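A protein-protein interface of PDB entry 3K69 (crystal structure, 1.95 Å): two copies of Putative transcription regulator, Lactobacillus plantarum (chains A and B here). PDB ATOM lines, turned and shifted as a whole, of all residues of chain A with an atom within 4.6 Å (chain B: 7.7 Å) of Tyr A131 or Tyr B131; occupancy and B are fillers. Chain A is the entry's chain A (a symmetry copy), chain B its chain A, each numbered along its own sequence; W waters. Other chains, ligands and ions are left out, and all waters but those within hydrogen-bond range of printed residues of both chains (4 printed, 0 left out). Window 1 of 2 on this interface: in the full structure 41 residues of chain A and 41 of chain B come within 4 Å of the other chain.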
ATOM      1  N   TYR A  83       1.420 -29.121 -22.025  1.00  0.00           N
ATOM      2  CA  TYR A  83       1.235 -27.794 -21.402  1.00  0.00           C
ATOM      3  C   TYR A  83       2.418 -27.493 -20.454  1.00  0.00           C
ATOM      4  O   TYR A  83       2.991 -26.411 -20.493  1.00  0.00           O
ATOM      5  CB  TYR A  83      -0.124 -27.692 -20.640  1.00  0.00           C
ATOM      6  CG  TYR A  83      -0.418 -26.279 -20.192  1.00  0.00           C
ATOM      7  CD1 TYR A  83       0.121 -25.772 -18.998  1.00  0.00           C
ATOM      8  CD2 TYR A  83      -1.163 -25.422 -20.996  1.00  0.00           C
ATOM      9  CE1 TYR A  83      -0.084 -24.452 -18.625  1.00  0.00           C
ATOM     10  CE2 TYR A  83      -1.386 -24.068 -20.621  1.00  0.00           C
ATOM     11  CZ  TYR A  83      -0.829 -23.595 -19.439  1.00  0.00           C
ATOM     12  OH  TYR A  83      -1.031 -22.280 -19.038  1.00  0.00           O
ATOM     13  N   ALA A 127      -3.300 -23.298  -6.509  1.00  0.00           N
ATOM     14  CA  ALA A 127      -4.256 -22.931  -7.538  1.00  0.00           C
ATOM     15  C   ALA A 127      -3.690 -23.340  -8.883  1.00  0.00           C
ATOM     16  O   ALA A 127      -4.406 -23.870  -9.700  1.00  0.00           O
ATOM     17  CB  ALA A 127      -4.555 -21.381  -7.525  1.00  0.00           C
ATOM     18  N   ASP A 128      -2.405 -23.093  -9.112  1.00  0.00           N
ATOM     19  CA  ASP A 128      -1.798 -23.448 -10.392  1.00  0.00           C
ATOM     20  C   ASP A 128      -1.777 -24.991 -10.607  1.00  0.00           C
ATOM     21  O   ASP A 128      -2.006 -25.459 -11.726  1.00  0.00           O
ATOM     22  CB  ASP A 128      -0.400 -22.845 -10.537  1.00  0.00           C
ATOM     23  CG  ASP A 128       0.177 -23.081 -11.923  1.00  0.00           C
ATOM     24  OD1 ASP A 128      -0.320 -22.450 -12.879  1.00  0.00           O
ATOM     25  OD2 ASP A 128       1.096 -23.914 -12.014  1.00  0.00           O
ATOM     26  N   ARG A 129      -1.613 -25.771  -9.545  1.00  0.00           N
ATOM     27  CA  ARG A 129      -1.701 -27.226  -9.691  1.00  0.00           C
ATOM     28  C   ARG A 129      -3.100 -27.646 -10.097  1.00  0.00           C
ATOM     29  O   ARG A 129      -3.248 -28.533 -10.911  1.00  0.00           O
ATOM     30  CB  ARG A 129      -1.239 -27.964  -8.423  1.00  0.00           C
ATOM     31  CG  ARG A 129       0.265 -28.003  -8.358  1.00  0.00           C
ATOM     32  CD  ARG A 129       0.758 -28.992  -7.385  1.00  0.00           C
ATOM     33  NE  ARG A 129       0.609 -28.540  -6.004  1.00  0.00           N
ATOM     34  CZ  ARG A 129       1.571 -27.947  -5.302  1.00  0.00           C
ATOM     35  NH1 ARG A 129       2.732 -27.653  -5.853  1.00  0.00           N
ATOM     36  NH2 ARG A 129       1.342 -27.594  -4.054  1.00  0.00           N
ATOM     37  N   GLN A 130      -4.124 -26.989  -9.548  1.00  0.00           N
ATOM     38  CA  GLN A 130      -5.515 -27.295  -9.908  1.00  0.00           C
ATOM     39  C   GLN A 130      -5.771 -26.937 -11.386  1.00  0.00           C
ATOM     40  O   GLN A 130      -6.403 -27.691 -12.121  1.00  0.00           O
ATOM     41  CB  GLN A 130      -6.481 -26.595  -8.954  1.00  0.00           C
ATOM     42  CG  GLN A 130      -7.956 -26.697  -9.378  1.00  0.00           C
ATOM     43  CD  GLN A 130      -8.944 -26.665  -8.215  1.00  0.00           C
ATOM     44  OE1 GLN A 130      -8.664 -27.230  -7.145  1.00  0.00           O
ATOM     45  NE2 GLN A 130     -10.126 -26.016  -8.426  1.00  0.00           N
ATOM     46  N   TYR A 131      -5.194 -25.837 -11.838  1.00  0.00           N
ATOM     47  CA  TYR A 131      -5.261 -25.441 -13.248  1.00  0.00           C
ATOM     48  C   TYR A 131      -4.628 -26.478 -14.146  1.00  0.00           C
ATOM     49  O   TYR A 131      -5.229 -26.914 -15.152  1.00  0.00           O
ATOM     50  CB  TYR A 131      -4.597 -24.069 -13.448  1.00  0.00           C
ATOM     51  CG  TYR A 131      -4.572 -23.556 -14.867  1.00  0.00           C
ATOM     52  CD1 TYR A 131      -5.721 -23.161 -15.479  1.00  0.00           C
ATOM     53  CD2 TYR A 131      -3.376 -23.436 -15.577  1.00  0.00           C
ATOM     54  CE1 TYR A 131      -5.717 -22.672 -16.784  1.00  0.00           C
ATOM     55  CE2 TYR A 131      -3.359 -22.977 -16.867  1.00  0.00           C
ATOM     56  CZ  TYR A 131      -4.540 -22.603 -17.479  1.00  0.00           C
ATOM     57  OH  TYR A 131      -4.590 -22.141 -18.772  1.00  0.00           O
ATOM     58  N   ARG A 132      -3.405 -26.878 -13.798  1.00  0.00           N
ATOM     59  CA  ARG A 132      -2.636 -27.784 -14.632  1.00  0.00           C
ATOM     60  C   ARG A 132      -3.241 -29.183 -14.640  1.00  0.00           C
ATOM     61  O   ARG A 132      -3.238 -29.828 -15.689  1.00  0.00           O
ATOM     62  CB  ARG A 132      -1.167 -27.775 -14.224  1.00  0.00           C
ATOM     63  CG  ARG A 132      -0.450 -26.500 -14.609  1.00  0.00           C
ATOM     64  CD  ARG A 132       0.961 -26.407 -14.035  1.00  0.00           C
ATOM     65  NE  ARG A 132       1.523 -25.112 -14.425  1.00  0.00           N
ATOM     66  CZ  ARG A 132       2.247 -24.895 -15.520  1.00  0.00           C
ATOM     67  NH1 ARG A 132       2.564 -25.887 -16.348  1.00  0.00           N
ATOM     68  NH2 ARG A 132       2.671 -23.665 -15.773  1.00  0.00           N
ATOM     69  N   ALA A 133      -3.840 -29.596 -13.517  1.00  0.00           N
ATOM     70  CA  ALA A 133      -4.611 -30.871 -13.410  1.00  0.00           C
ATOM     71  C   ALA A 133      -5.682 -30.975 -14.494  1.00  0.00           C
ATOM     72  O   ALA A 133      -5.971 -32.063 -14.991  1.00  0.00           O
ATOM     73  CB  ALA A 133      -5.273 -31.043 -11.969  1.00  0.00           C
ATOM     74  N   TYR A 134      -6.282 -29.849 -14.859  1.00  0.00           N
ATOM     75  CA  TYR A 134      -7.316 -29.858 -15.898  1.00  0.00           C
ATOM     76  C   TYR A 134      -6.796 -30.490 -17.215  1.00  0.00           C
ATOM     77  O   TYR A 134      -7.425 -31.407 -17.770  1.00  0.00           O
ATOM     78  CB  TYR A 134      -7.886 -28.453 -16.161  1.00  0.00           C
ATOM     79  CG  TYR A 134      -8.778 -28.425 -17.374  1.00  0.00           C
ATOM     80  CD1 TYR A 134     -10.076 -28.954 -17.310  1.00  0.00           C
ATOM     81  CD2 TYR A 134      -8.301 -27.996 -18.596  1.00  0.00           C
ATOM     82  CE1 TYR A 134     -10.866 -28.996 -18.411  1.00  0.00           C
ATOM     83  CE2 TYR A 134      -9.111 -28.006 -19.701  1.00  0.00           C
ATOM     84  CZ  TYR A 134     -10.395 -28.517 -19.599  1.00  0.00           C
ATOM     85  OH  TYR A 134     -11.200 -28.565 -20.704  1.00  0.00           O
ATOM     86  N   TYR A 135      -5.649 -30.016 -17.689  1.00  0.00           N
ATOM     87  CA  TYR A 135      -5.090 -30.489 -18.953  1.00  0.00           C
ATOM     88  C   TYR A 135      -4.637 -31.939 -18.882  1.00  0.00           C
ATOM     89  O   TYR A 135      -4.771 -32.659 -19.862  1.00  0.00           O
ATOM     90  CB  TYR A 135      -3.946 -29.605 -19.400  1.00  0.00           C
ATOM     91  CG  TYR A 135      -4.304 -28.152 -19.653  1.00  0.00           C
ATOM     92  CD1 TYR A 135      -4.795 -27.752 -20.886  1.00  0.00           C
ATOM     93  CD2 TYR A 135      -4.076 -27.182 -18.703  1.00  0.00           C
ATOM     94  CE1 TYR A 135      -5.063 -26.463 -21.137  1.00  0.00           C
ATOM     95  CE2 TYR A 135      -4.372 -25.865 -18.951  1.00  0.00           C
ATOM     96  CZ  TYR A 135      -4.871 -25.514 -20.172  1.00  0.00           C
ATOM     97  OH  TYR A 135      -5.152 -24.221 -20.486  1.00  0.00           O
ATOM     98  N   LYS B   8      -1.853  -8.187 -12.748  1.00  0.00           N
ATOM     99  CA  LYS B   8      -2.200  -9.357 -11.916  1.00  0.00           C
ATOM    100  C   LYS B   8      -1.720  -9.157 -10.445  1.00  0.00           C
ATOM    101  O   LYS B   8      -2.219  -9.833  -9.521  1.00  0.00           O
ATOM    102  CB  LYS B   8      -1.653 -10.633 -12.524  1.00  0.00           C
ATOM    103  CG  LYS B   8      -2.447 -11.117 -13.739  1.00  0.00           C
ATOM    104  CD  LYS B   8      -2.244 -12.638 -13.976  1.00  0.00           C
ATOM    105  CE  LYS B   8      -0.868 -12.940 -14.615  1.00  0.00           C
ATOM    106  N   PHE B  11      -4.559  -8.402  -7.374  1.00  0.00           N
ATOM    107  CA  PHE B  11      -5.125  -9.291  -6.376  1.00  0.00           C
ATOM    108  C   PHE B  11      -4.379  -9.140  -5.033  1.00  0.00           C
ATOM    109  O   PHE B  11      -5.001  -8.936  -3.968  1.00  0.00           O
ATOM    110  CB  PHE B  11      -5.106 -10.748  -6.844  1.00  0.00           C
ATOM    111  CG  PHE B  11      -5.665 -11.742  -5.807  1.00  0.00           C
ATOM    112  CD1 PHE B  11      -7.015 -11.743  -5.491  1.00  0.00           C
ATOM    113  CD2 PHE B  11      -4.859 -12.678  -5.214  1.00  0.00           C
ATOM    114  CE1 PHE B  11      -7.525 -12.627  -4.560  1.00  0.00           C
ATOM    115  CE2 PHE B  11      -5.377 -13.596  -4.317  1.00  0.00           C
ATOM    116  CZ  PHE B  11      -6.720 -13.557  -3.988  1.00  0.00           C
ATOM    117  N   TYR B  83     -10.829 -12.374  -6.256  1.00  0.00           N
ATOM    118  CA  TYR B  83      -9.944 -12.707  -7.391  1.00  0.00           C
ATOM    119  C   TYR B  83     -10.610 -12.273  -8.717  1.00  0.00           C
ATOM    120  O   TYR B  83      -9.978 -11.645  -9.558  1.00  0.00           O
ATOM    121  CB  TYR B  83      -9.583 -14.225  -7.424  1.00  0.00           C
ATOM    122  CG  TYR B  83      -8.509 -14.530  -8.442  1.00  0.00           C
ATOM    123  CD1 TYR B  83      -8.830 -14.729  -9.795  1.00  0.00           C
ATOM    124  CD2 TYR B  83      -7.167 -14.540  -8.074  1.00  0.00           C
ATOM    125  CE1 TYR B  83      -7.839 -14.931 -10.743  1.00  0.00           C
ATOM    126  CE2 TYR B  83      -6.141 -14.755  -9.035  1.00  0.00           C
ATOM    127  CZ  TYR B  83      -6.492 -14.936 -10.367  1.00  0.00           C
ATOM    128  OH  TYR B  83      -5.517 -15.154 -11.333  1.00  0.00           O
ATOM    129  N   ASP B  84     -11.885 -12.629  -8.874  1.00  0.00           N
ATOM    130  CA  ASP B  84     -12.613 -12.358 -10.087  1.00  0.00           C
ATOM    131  C   ASP B  84     -12.779 -10.857 -10.296  1.00  0.00           C
ATOM    132  O   ASP B  84     -12.693 -10.372 -11.438  1.00  0.00           O
ATOM    133  CB  ASP B  84     -13.968 -13.080 -10.118  1.00  0.00           C
ATOM    134  CG  ASP B  84     -13.854 -14.612 -10.114  1.00  0.00           C
ATOM    135  OD1 ASP B  84     -12.771 -15.213 -10.399  1.00  0.00           O
ATOM    136  OD2 ASP B  84     -14.891 -15.225  -9.778  1.00  0.00           O
ATOM    137  N   ILE B  87      -8.954  -9.484 -10.951  1.00  0.00           N
ATOM    138  CA  ILE B  87      -8.344 -10.056 -12.159  1.00  0.00           C
ATOM    139  C   ILE B  87      -9.493 -10.583 -13.024  1.00  0.00           C
ATOM    140  O   ILE B  87      -9.760 -11.755 -13.019  1.00  0.00           O
ATOM    141  CB  ILE B  87      -7.270 -11.146 -11.824  1.00  0.00           C
ATOM    142  CG1 ILE B  87      -6.173 -10.549 -10.938  1.00  0.00           C
ATOM    143  CG2 ILE B  87      -6.599 -11.705 -13.115  1.00  0.00           C
ATOM    144  CD1 ILE B  87      -5.138 -11.508 -10.543  1.00  0.00           C
ATOM    145  N   TYR B  93      -8.953 -15.074 -26.047  1.00  0.00           N
ATOM    146  CA  TYR B  93      -7.621 -15.681 -25.885  1.00  0.00           C
ATOM    147  C   TYR B  93      -6.783 -15.539 -27.165  1.00  0.00           C
ATOM    148  O   TYR B  93      -5.761 -16.226 -27.314  1.00  0.00           O
ATOM    149  CB  TYR B  93      -7.755 -17.157 -25.488  1.00  0.00           C
ATOM    150  CG  TYR B  93      -8.167 -17.375 -24.067  1.00  0.00           C
ATOM    151  CD1 TYR B  93      -7.218 -17.363 -23.045  1.00  0.00           C
ATOM    152  CD2 TYR B  93      -9.508 -17.502 -23.720  1.00  0.00           C
ATOM    153  CE1 TYR B  93      -7.582 -17.543 -21.716  1.00  0.00           C
ATOM    154  CE2 TYR B  93      -9.885 -17.695 -22.402  1.00  0.00           C
ATOM    155  CZ  TYR B  93      -8.915 -17.692 -21.401  1.00  0.00           C
ATOM    156  OH  TYR B  93      -9.262 -17.849 -20.085  1.00  0.00           O
ATOM    157  N   LEU B 123     -11.028 -24.821 -24.597  1.00  0.00           N
ATOM    158  CA  LEU B 123     -10.042 -25.424 -23.727  1.00  0.00           C
ATOM    159  C   LEU B 123      -9.557 -24.461 -22.589  1.00  0.00           C
ATOM    160  O   LEU B 123      -9.655 -24.785 -21.400  1.00  0.00           O
ATOM    161  CB  LEU B 123      -8.869 -25.946 -24.543  1.00  0.00           C
ATOM    162  CG  LEU B 123      -7.810 -26.757 -23.766  1.00  0.00           C
ATOM    163  CD1 LEU B 123      -8.336 -28.095 -23.250  1.00  0.00           C
ATOM    164  CD2 LEU B 123      -6.490 -26.920 -24.548  1.00  0.00           C
ATOM    165  N   PHE B 124      -9.038 -23.303 -22.987  1.00  0.00           N
ATOM    166  CA  PHE B 124      -8.512 -22.273 -22.072  1.00  0.00           C
ATOM    167  C   PHE B 124      -9.606 -21.717 -21.158  1.00  0.00           C
ATOM    168  O   PHE B 124      -9.364 -21.463 -19.980  1.00  0.00           O
ATOM    169  CB  PHE B 124      -7.929 -21.104 -22.869  1.00  0.00           C
ATOM    170  CG  PHE B 124      -6.701 -21.425 -23.668  1.00  0.00           C
ATOM    171  CD1 PHE B 124      -5.807 -22.416 -23.285  1.00  0.00           C
ATOM    172  CD2 PHE B 124      -6.402 -20.698 -24.793  1.00  0.00           C
ATOM    173  CE1 PHE B 124      -4.634 -22.670 -24.053  1.00  0.00           C
ATOM    174  CE2 PHE B 124      -5.251 -20.952 -25.562  1.00  0.00           C
ATOM    175  CZ  PHE B 124      -4.368 -21.936 -25.168  1.00  0.00           C
ATOM    176  N   THR B 125     -10.820 -21.546 -21.691  1.00  0.00           N
ATOM    177  CA  THR B 125     -11.943 -21.048 -20.884  1.00  0.00           C
ATOM    178  C   THR B 125     -12.380 -22.041 -19.828  1.00  0.00           C
ATOM    179  O   THR B 125     -12.579 -21.671 -18.666  1.00  0.00           O
ATOM    180  CB  THR B 125     -13.144 -20.618 -21.752  1.00  0.00           C
ATOM    181  OG1 THR B 125     -12.685 -19.702 -22.753  1.00  0.00           O
ATOM    182  CG2 THR B 125     -14.232 -19.946 -20.903  1.00  0.00           C
ATOM    183  N   VAL B 126     -12.542 -23.305 -20.199  1.00  0.00           N
ATOM    184  CA  VAL B 126     -12.869 -24.317 -19.207  1.00  0.00           C
ATOM    185  C   VAL B 126     -11.768 -24.422 -18.124  1.00  0.00           C
ATOM    186  O   VAL B 126     -12.069 -24.530 -16.921  1.00  0.00           O
ATOM    187  CB  VAL B 126     -13.156 -25.705 -19.888  1.00  0.00           C
ATOM    188  CG1 VAL B 126     -13.383 -26.766 -18.845  1.00  0.00           C
ATOM    189  CG2 VAL B 126     -14.411 -25.581 -20.845  1.00  0.00           C
ATOM    190  N   ALA B 127     -10.500 -24.429 -18.565  1.00  0.00           N
ATOM    191  CA  ALA B 127      -9.366 -24.542 -17.666  1.00  0.00           C
ATOM    192  C   ALA B 127      -9.387 -23.359 -16.720  1.00  0.00           C
ATOM    193  O   ALA B 127      -9.162 -23.527 -15.544  1.00  0.00           O
ATOM    194  CB  ALA B 127      -8.001 -24.579 -18.458  1.00  0.00           C
ATOM    195  N   ASP B 128      -9.656 -22.165 -17.233  1.00  0.00           N
ATOM    196  CA  ASP B 128      -9.677 -20.978 -16.381  1.00  0.00           C
ATOM    197  C   ASP B 128     -10.832 -21.045 -15.337  1.00  0.00           C
ATOM    198  O   ASP B 128     -10.646 -20.638 -14.187  1.00  0.00           O
ATOM    199  CB  ASP B 128      -9.745 -19.693 -17.207  1.00  0.00           C
ATOM    200  CG  ASP B 128      -9.615 -18.454 -16.337  1.00  0.00           C
ATOM    201  OD1 ASP B 128      -8.500 -18.207 -15.833  1.00  0.00           O
ATOM    202  OD2 ASP B 128     -10.645 -17.779 -16.166  1.00  0.00           O
ATOM    203  N   ARG B 129     -11.966 -21.640 -15.691  1.00  0.00           N
ATOM    204  CA  ARG B 129     -13.031 -21.822 -14.703  1.00  0.00           C
ATOM    205  C   ARG B 129     -12.589 -22.761 -13.597  1.00  0.00           C
ATOM    206  O   ARG B 129     -12.899 -22.524 -12.449  1.00  0.00           O
ATOM    207  CB  ARG B 129     -14.345 -22.294 -15.348  1.00  0.00           C
ATOM    208  CG  ARG B 129     -15.059 -21.134 -15.990  1.00  0.00           C
ATOM    209  CD  ARG B 129     -16.467 -21.442 -16.295  1.00  0.00           C
ATOM    210  NE  ARG B 129     -16.608 -22.307 -17.463  1.00  0.00           N
ATOM    211  CZ  ARG B 129     -16.843 -21.868 -18.697  1.00  0.00           C
ATOM    212  NH1 ARG B 129     -16.887 -20.577 -18.962  1.00  0.00           N
ATOM    213  NH2 ARG B 129     -16.974 -22.732 -19.682  1.00  0.00           N
ATOM    214  N   GLN B 130     -11.843 -23.812 -13.943  1.00  0.00           N
ATOM    215  CA  GLN B 130     -11.333 -24.756 -12.940  1.00  0.00           C
ATOM    216  C   GLN B 130     -10.326 -24.049 -12.010  1.00  0.00           C
ATOM    217  O   GLN B 130     -10.351 -24.227 -10.795  1.00  0.00           O
ATOM    218  CB  GLN B 130     -10.744 -25.993 -13.618  1.00  0.00           C
ATOM    219  CG  GLN B 130     -10.007 -26.938 -12.655  1.00  0.00           C
ATOM    220  CD  GLN B 130     -10.030 -28.404 -13.080  1.00  0.00           C
ATOM    221  OE1 GLN B 130     -11.044 -28.881 -13.613  1.00  0.00           O
ATOM    222  NE2 GLN B 130      -8.908 -29.139 -12.825  1.00  0.00           N
ATOM    223  N   TYR B 131      -9.512 -23.175 -12.574  1.00  0.00           N
ATOM    224  CA  TYR B 131      -8.585 -22.350 -11.792  1.00  0.00           C
ATOM    225  C   TYR B 131      -9.321 -21.460 -10.820  1.00  0.00           C
ATOM    226  O   TYR B 131      -8.994 -21.412  -9.614  1.00  0.00           O
ATOM    227  CB  TYR B 131      -7.694 -21.516 -12.728  1.00  0.00           C
ATOM    228  CG  TYR B 131      -6.711 -20.597 -12.046  1.00  0.00           C
ATOM    229  CD1 TYR B 131      -5.641 -21.105 -11.375  1.00  0.00           C
ATOM    230  CD2 TYR B 131      -6.844 -19.209 -12.112  1.00  0.00           C
ATOM    231  CE1 TYR B 131      -4.714 -20.273 -10.751  1.00  0.00           C
ATOM    232  CE2 TYR B 131      -5.953 -18.380 -11.486  1.00  0.00           C
ATOM    233  CZ  TYR B 131      -4.886 -18.916 -10.790  1.00  0.00           C
ATOM    234  OH  TYR B 131      -3.963 -18.138 -10.135  1.00  0.00           O
ATOM    235  N   ARG B 132     -10.317 -20.739 -11.333  1.00  0.00           N
ATOM    236  CA  ARG B 132     -11.035 -19.758 -10.537  1.00  0.00           C
ATOM    237  C   ARG B 132     -11.887 -20.427  -9.465  1.00  0.00           C
ATOM    238  O   ARG B 132     -11.973 -19.899  -8.355  1.00  0.00           O
ATOM    239  CB  ARG B 132     -11.836 -18.820 -11.432  1.00  0.00           C
ATOM    240  CG  ARG B 132     -10.971 -17.849 -12.203  1.00  0.00           C
ATOM    241  CD  ARG B 132     -11.748 -17.043 -13.240  1.00  0.00           C
ATOM    242  NE  ARG B 132     -10.797 -16.190 -13.956  1.00  0.00           N
ATOM    243  CZ  ARG B 132     -10.488 -14.941 -13.615  1.00  0.00           C
ATOM    244  NH1 ARG B 132     -11.079 -14.338 -12.587  1.00  0.00           N
ATOM    245  NH2 ARG B 132      -9.585 -14.287 -14.332  1.00  0.00           N
ATOM    246  N   ALA B 133     -12.419 -21.619  -9.762  1.00  0.00           N
ATOM    247  CA  ALA B 133     -13.146 -22.471  -8.774  1.00  0.00           C
ATOM    248  C   ALA B 133     -12.315 -22.709  -7.514  1.00  0.00           C
ATOM    249  O   ALA B 133     -12.855 -22.796  -6.412  1.00  0.00           O
ATOM    250  CB  ALA B 133     -13.588 -23.866  -9.408  1.00  0.00           C
ATOM    251  N   TYR B 134     -11.003 -22.823  -7.670  1.00  0.00           N
ATOM    252  CA  TYR B 134     -10.131 -23.044  -6.512  1.00  0.00           C
ATOM    253  C   TYR B 134     -10.321 -21.944  -5.436  1.00  0.00           C
ATOM    254  O   TYR B 134     -10.551 -22.247  -4.253  1.00  0.00           O
ATOM    255  CB  TYR B 134      -8.650 -23.156  -6.915  1.00  0.00           C
ATOM    256  CG  TYR B 134      -7.739 -23.157  -5.716  1.00  0.00           C
ATOM    257  CD1 TYR B 134      -7.623 -24.304  -4.917  1.00  0.00           C
ATOM    258  CD2 TYR B 134      -7.100 -22.003  -5.308  1.00  0.00           C
ATOM    259  CE1 TYR B 134      -6.858 -24.298  -3.797  1.00  0.00           C
ATOM    260  CE2 TYR B 134      -6.300 -22.007  -4.196  1.00  0.00           C
ATOM    261  CZ  TYR B 134      -6.190 -23.162  -3.440  1.00  0.00           C
ATOM    262  OH  TYR B 134      -5.423 -23.167  -2.308  1.00  0.00           O
ATOM    263  N   TYR B 135     -10.247 -20.685  -5.853  1.00  0.00           N
ATOM    264  CA  TYR B 135     -10.349 -19.563  -4.924  1.00  0.00           C
ATOM    265  C   TYR B 135     -11.736 -19.439  -4.312  1.00  0.00           C
ATOM    266  O   TYR B 135     -11.850 -19.070  -3.152  1.00  0.00           O
ATOM    267  CB  TYR B 135      -9.956 -18.266  -5.599  1.00  0.00           C
ATOM    268  CG  TYR B 135      -8.534 -18.209  -6.124  1.00  0.00           C
ATOM    269  CD1 TYR B 135      -7.492 -17.826  -5.293  1.00  0.00           C
ATOM    270  CD2 TYR B 135      -8.248 -18.450  -7.449  1.00  0.00           C
ATOM    271  CE1 TYR B 135      -6.240 -17.719  -5.761  1.00  0.00           C
ATOM    272  CE2 TYR B 135      -6.964 -18.363  -7.923  1.00  0.00           C
ATOM    273  CZ  TYR B 135      -5.962 -18.002  -7.069  1.00  0.00           C
ATOM    274  OH  TYR B 135      -4.676 -17.868  -7.489  1.00  0.00           O
ATOM    275  N   HIS B 136     -12.783 -19.826  -5.049  1.00  0.00           N
ATOM    276  CA  HIS B 136     -14.133 -19.773  -4.497  1.00  0.00           C
ATOM    277  C   HIS B 136     -14.426 -20.654  -3.285  1.00  0.00           C
ATOM    278  O   HIS B 136     -15.438 -20.428  -2.602  1.00  0.00           O
ATOM    279  CB  HIS B 136     -15.197 -19.999  -5.595  1.00  0.00           C
ATOM    280  CG  HIS B 136     -15.400 -18.799  -6.451  1.00  0.00           C
ATOM    281  ND1 HIS B 136     -16.274 -17.791  -6.119  1.00  0.00           N
ATOM    282  CD2 HIS B 136     -14.743 -18.373  -7.553  1.00  0.00           C
ATOM    283  CE1 HIS B 136     -16.218 -16.840  -7.036  1.00  0.00           C
ATOM    284  NE2 HIS B 136     -15.278 -17.160  -7.901  1.00  0.00           N
ATOM    285  N   GLN B 137     -13.560 -21.632  -3.022  1.00  0.00           N
ATOM    286  CA  GLN B 137     -13.639 -22.457  -1.830  1.00  0.00           C
ATOM    287  C   GLN B 137     -13.345 -21.707  -0.552  1.00  0.00           C
ATOM    288  O   GLN B 137     -13.689 -22.203   0.504  1.00  0.00           O
ATOM    289  CB  GLN B 137     -12.629 -23.609  -1.848  1.00  0.00           C
ATOM    290  CG  GLN B 137     -12.677 -24.525  -3.040  1.00  0.00           C
ATOM    291  CD  GLN B 137     -11.529 -25.481  -2.994  1.00  0.00           C
ATOM    292  OE1 GLN B 137     -10.393 -25.124  -3.311  1.00  0.00           O
ATOM    293  NE2 GLN B 137     -11.807 -26.700  -2.551  1.00  0.00           N
HETATM  294  O   HOH W   1     -12.081 -26.196  -6.554  1.00  0.00           O
HETATM  295  O   HOH W   2      -8.970 -31.821 -13.224  1.00  0.00           O
HETATM  296  O   HOH W   3      -6.762 -20.638 -19.454  1.00  0.00           O
HETATM  297  O   HOH W   4      -9.085 -27.626  -4.527  1.00  0.00           O
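Hydrophobic or aromatic side chains of chain B that line the printed part of chain A: Leu B123, Phe B124, Val B126, Ala B127, Tyr B131, Tyr B134 and Tyr B135. Printed residues of chain A that touch a printed residue of chain B: Ala A127, Asp A128, Gln A130, Tyr A131, Tyr A134 and Tyr A135. Hydrophobic or aromatic side chains of chain A that line the printed part of chain B: Ala A127, Tyr A131, Tyr A134 and Tyr A135. Along chain A the printed residues that touch a printed residue of chain B span positions 127 to 135. Among the printed residues, 16 pairs touch across the chains. Among the printed residues, no Asp or Glu carboxylate lies within 4 Å of a Lys or Arg side-chain nitrogen of the other chain.
Of the printed residues of chain B, Tyr A131 touches Ala B127, Asp B128 and Tyr B131. Of the printed residues of chain A, Tyr B131 touches Ala A127 (3.4 Å), Asp A128 (3.996 Å) and Tyr A131 (3.8 Å). Of the printed residues of chain A, Tyr B135 touches Ala A127. Of the printed residues of chain A, Gln B130 touches Gln A130 and Tyr A134. Printed residues of chain B within 4 Å of Tyr A134: Leu B123, Val B126, Ala B127 and Gln B130. Of the printed residues of chain B, Ala A127 touches Tyr B131 (3.4 Å), Tyr B134 (3.4 Å) and Tyr B135 (3.5 Å). Of the printed residues of chain B, Tyr A135 touches Leu B123, Phe B124 and Ala B127. Ala B133 touches none of the printed residues of chain A. The nearest printed residue of chain B that does not touch Tyr A131 is Phe B124 (4.7 Å). The nearest printed residue of chain A that does not touch Leu B123 is Tyr A131 (6.3 Å).
The side-chain amide nitrogen (NE2) of Gln A130 sits at hydrogen-bond distance from the backbone carbonyl oxygen (O) of Gln B130, 3.0 Å away. The side-chain amide nitrogen of Gln A130 sits close to the backbone NH of Tyr B134 (3.4 Å). NE2 of Gln B130 lies close to N of Tyr A134 (3.4 Å).
Among the printed residues, pairs that only touch across the chains: Tyr A134 with Val B126, Tyr A135 with Phe B124, Tyr A131 with Ala B127, Ala A127 with Tyr B131, Ala A127 with Tyr B134, Tyr A134 with Ala B127, Ala A127 with Tyr B135, Tyr A135 with Ala B127, Tyr A134 with Leu B123, Tyr A135 with Leu B123, Tyr A131 with Tyr B131, Asp A128 with Tyr B131 and Tyr A131 with Asp B128.
The side-chain carboxylate of Asp A128 lies within salt-bridge range of the guanidinium group of Arg A132 (2.7 Å). The guanidinium group (NE) of Arg B132 lies within salt-bridge range of the side-chain carboxylate (OD2) of Asp B128 (2.7 Å). The side-chain hydroxyl (OH) of Tyr A131 lies within hydrogen-bond range of the side-chain hydroxyl (OH) of Tyr A135 (2.8 Å). OE1 of Gln B137 sits close to O of Tyr B134, at 3.0 Å. OH of Tyr B135 lies within hydrogen-bond range of OH of Tyr B131, 2.8 Å away.
Ala A127 touches Tyr B131, and with the chains exchanged Tyr A131 touches Ala B127. Ala A127 touches Tyr B134, and with the chains exchanged Tyr A134 touches Ala B127. Ala A127 touches Tyr B135, and with the chains exchanged Tyr A135 touches Ala B127. Tyr A131 touches its own counterpart, Tyr B131. Of the 16 pairs that touch across the chains among the printed residues, 12 have their exchanged pair printed and touching as well.
Water W4 bridges OE1 of Gln A130 (2.7 Å) and OE1 of Gln B137 (3.1 Å). Water W2 lies within hydrogen-bond range of the side-chain amide nitrogen of Gln B130 and the backbone carbonyl oxygen of Ala A133. Water W1 bridges the side-chain amide nitrogen (NE2) of Gln A130 (2.7 Å) and the backbone carbonyl oxygen (O) of Ala B133 (3.5 Å). Water W3 bridges OH of Tyr A131 (2.7 Å) and O of Phe B124 (2.8 Å).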
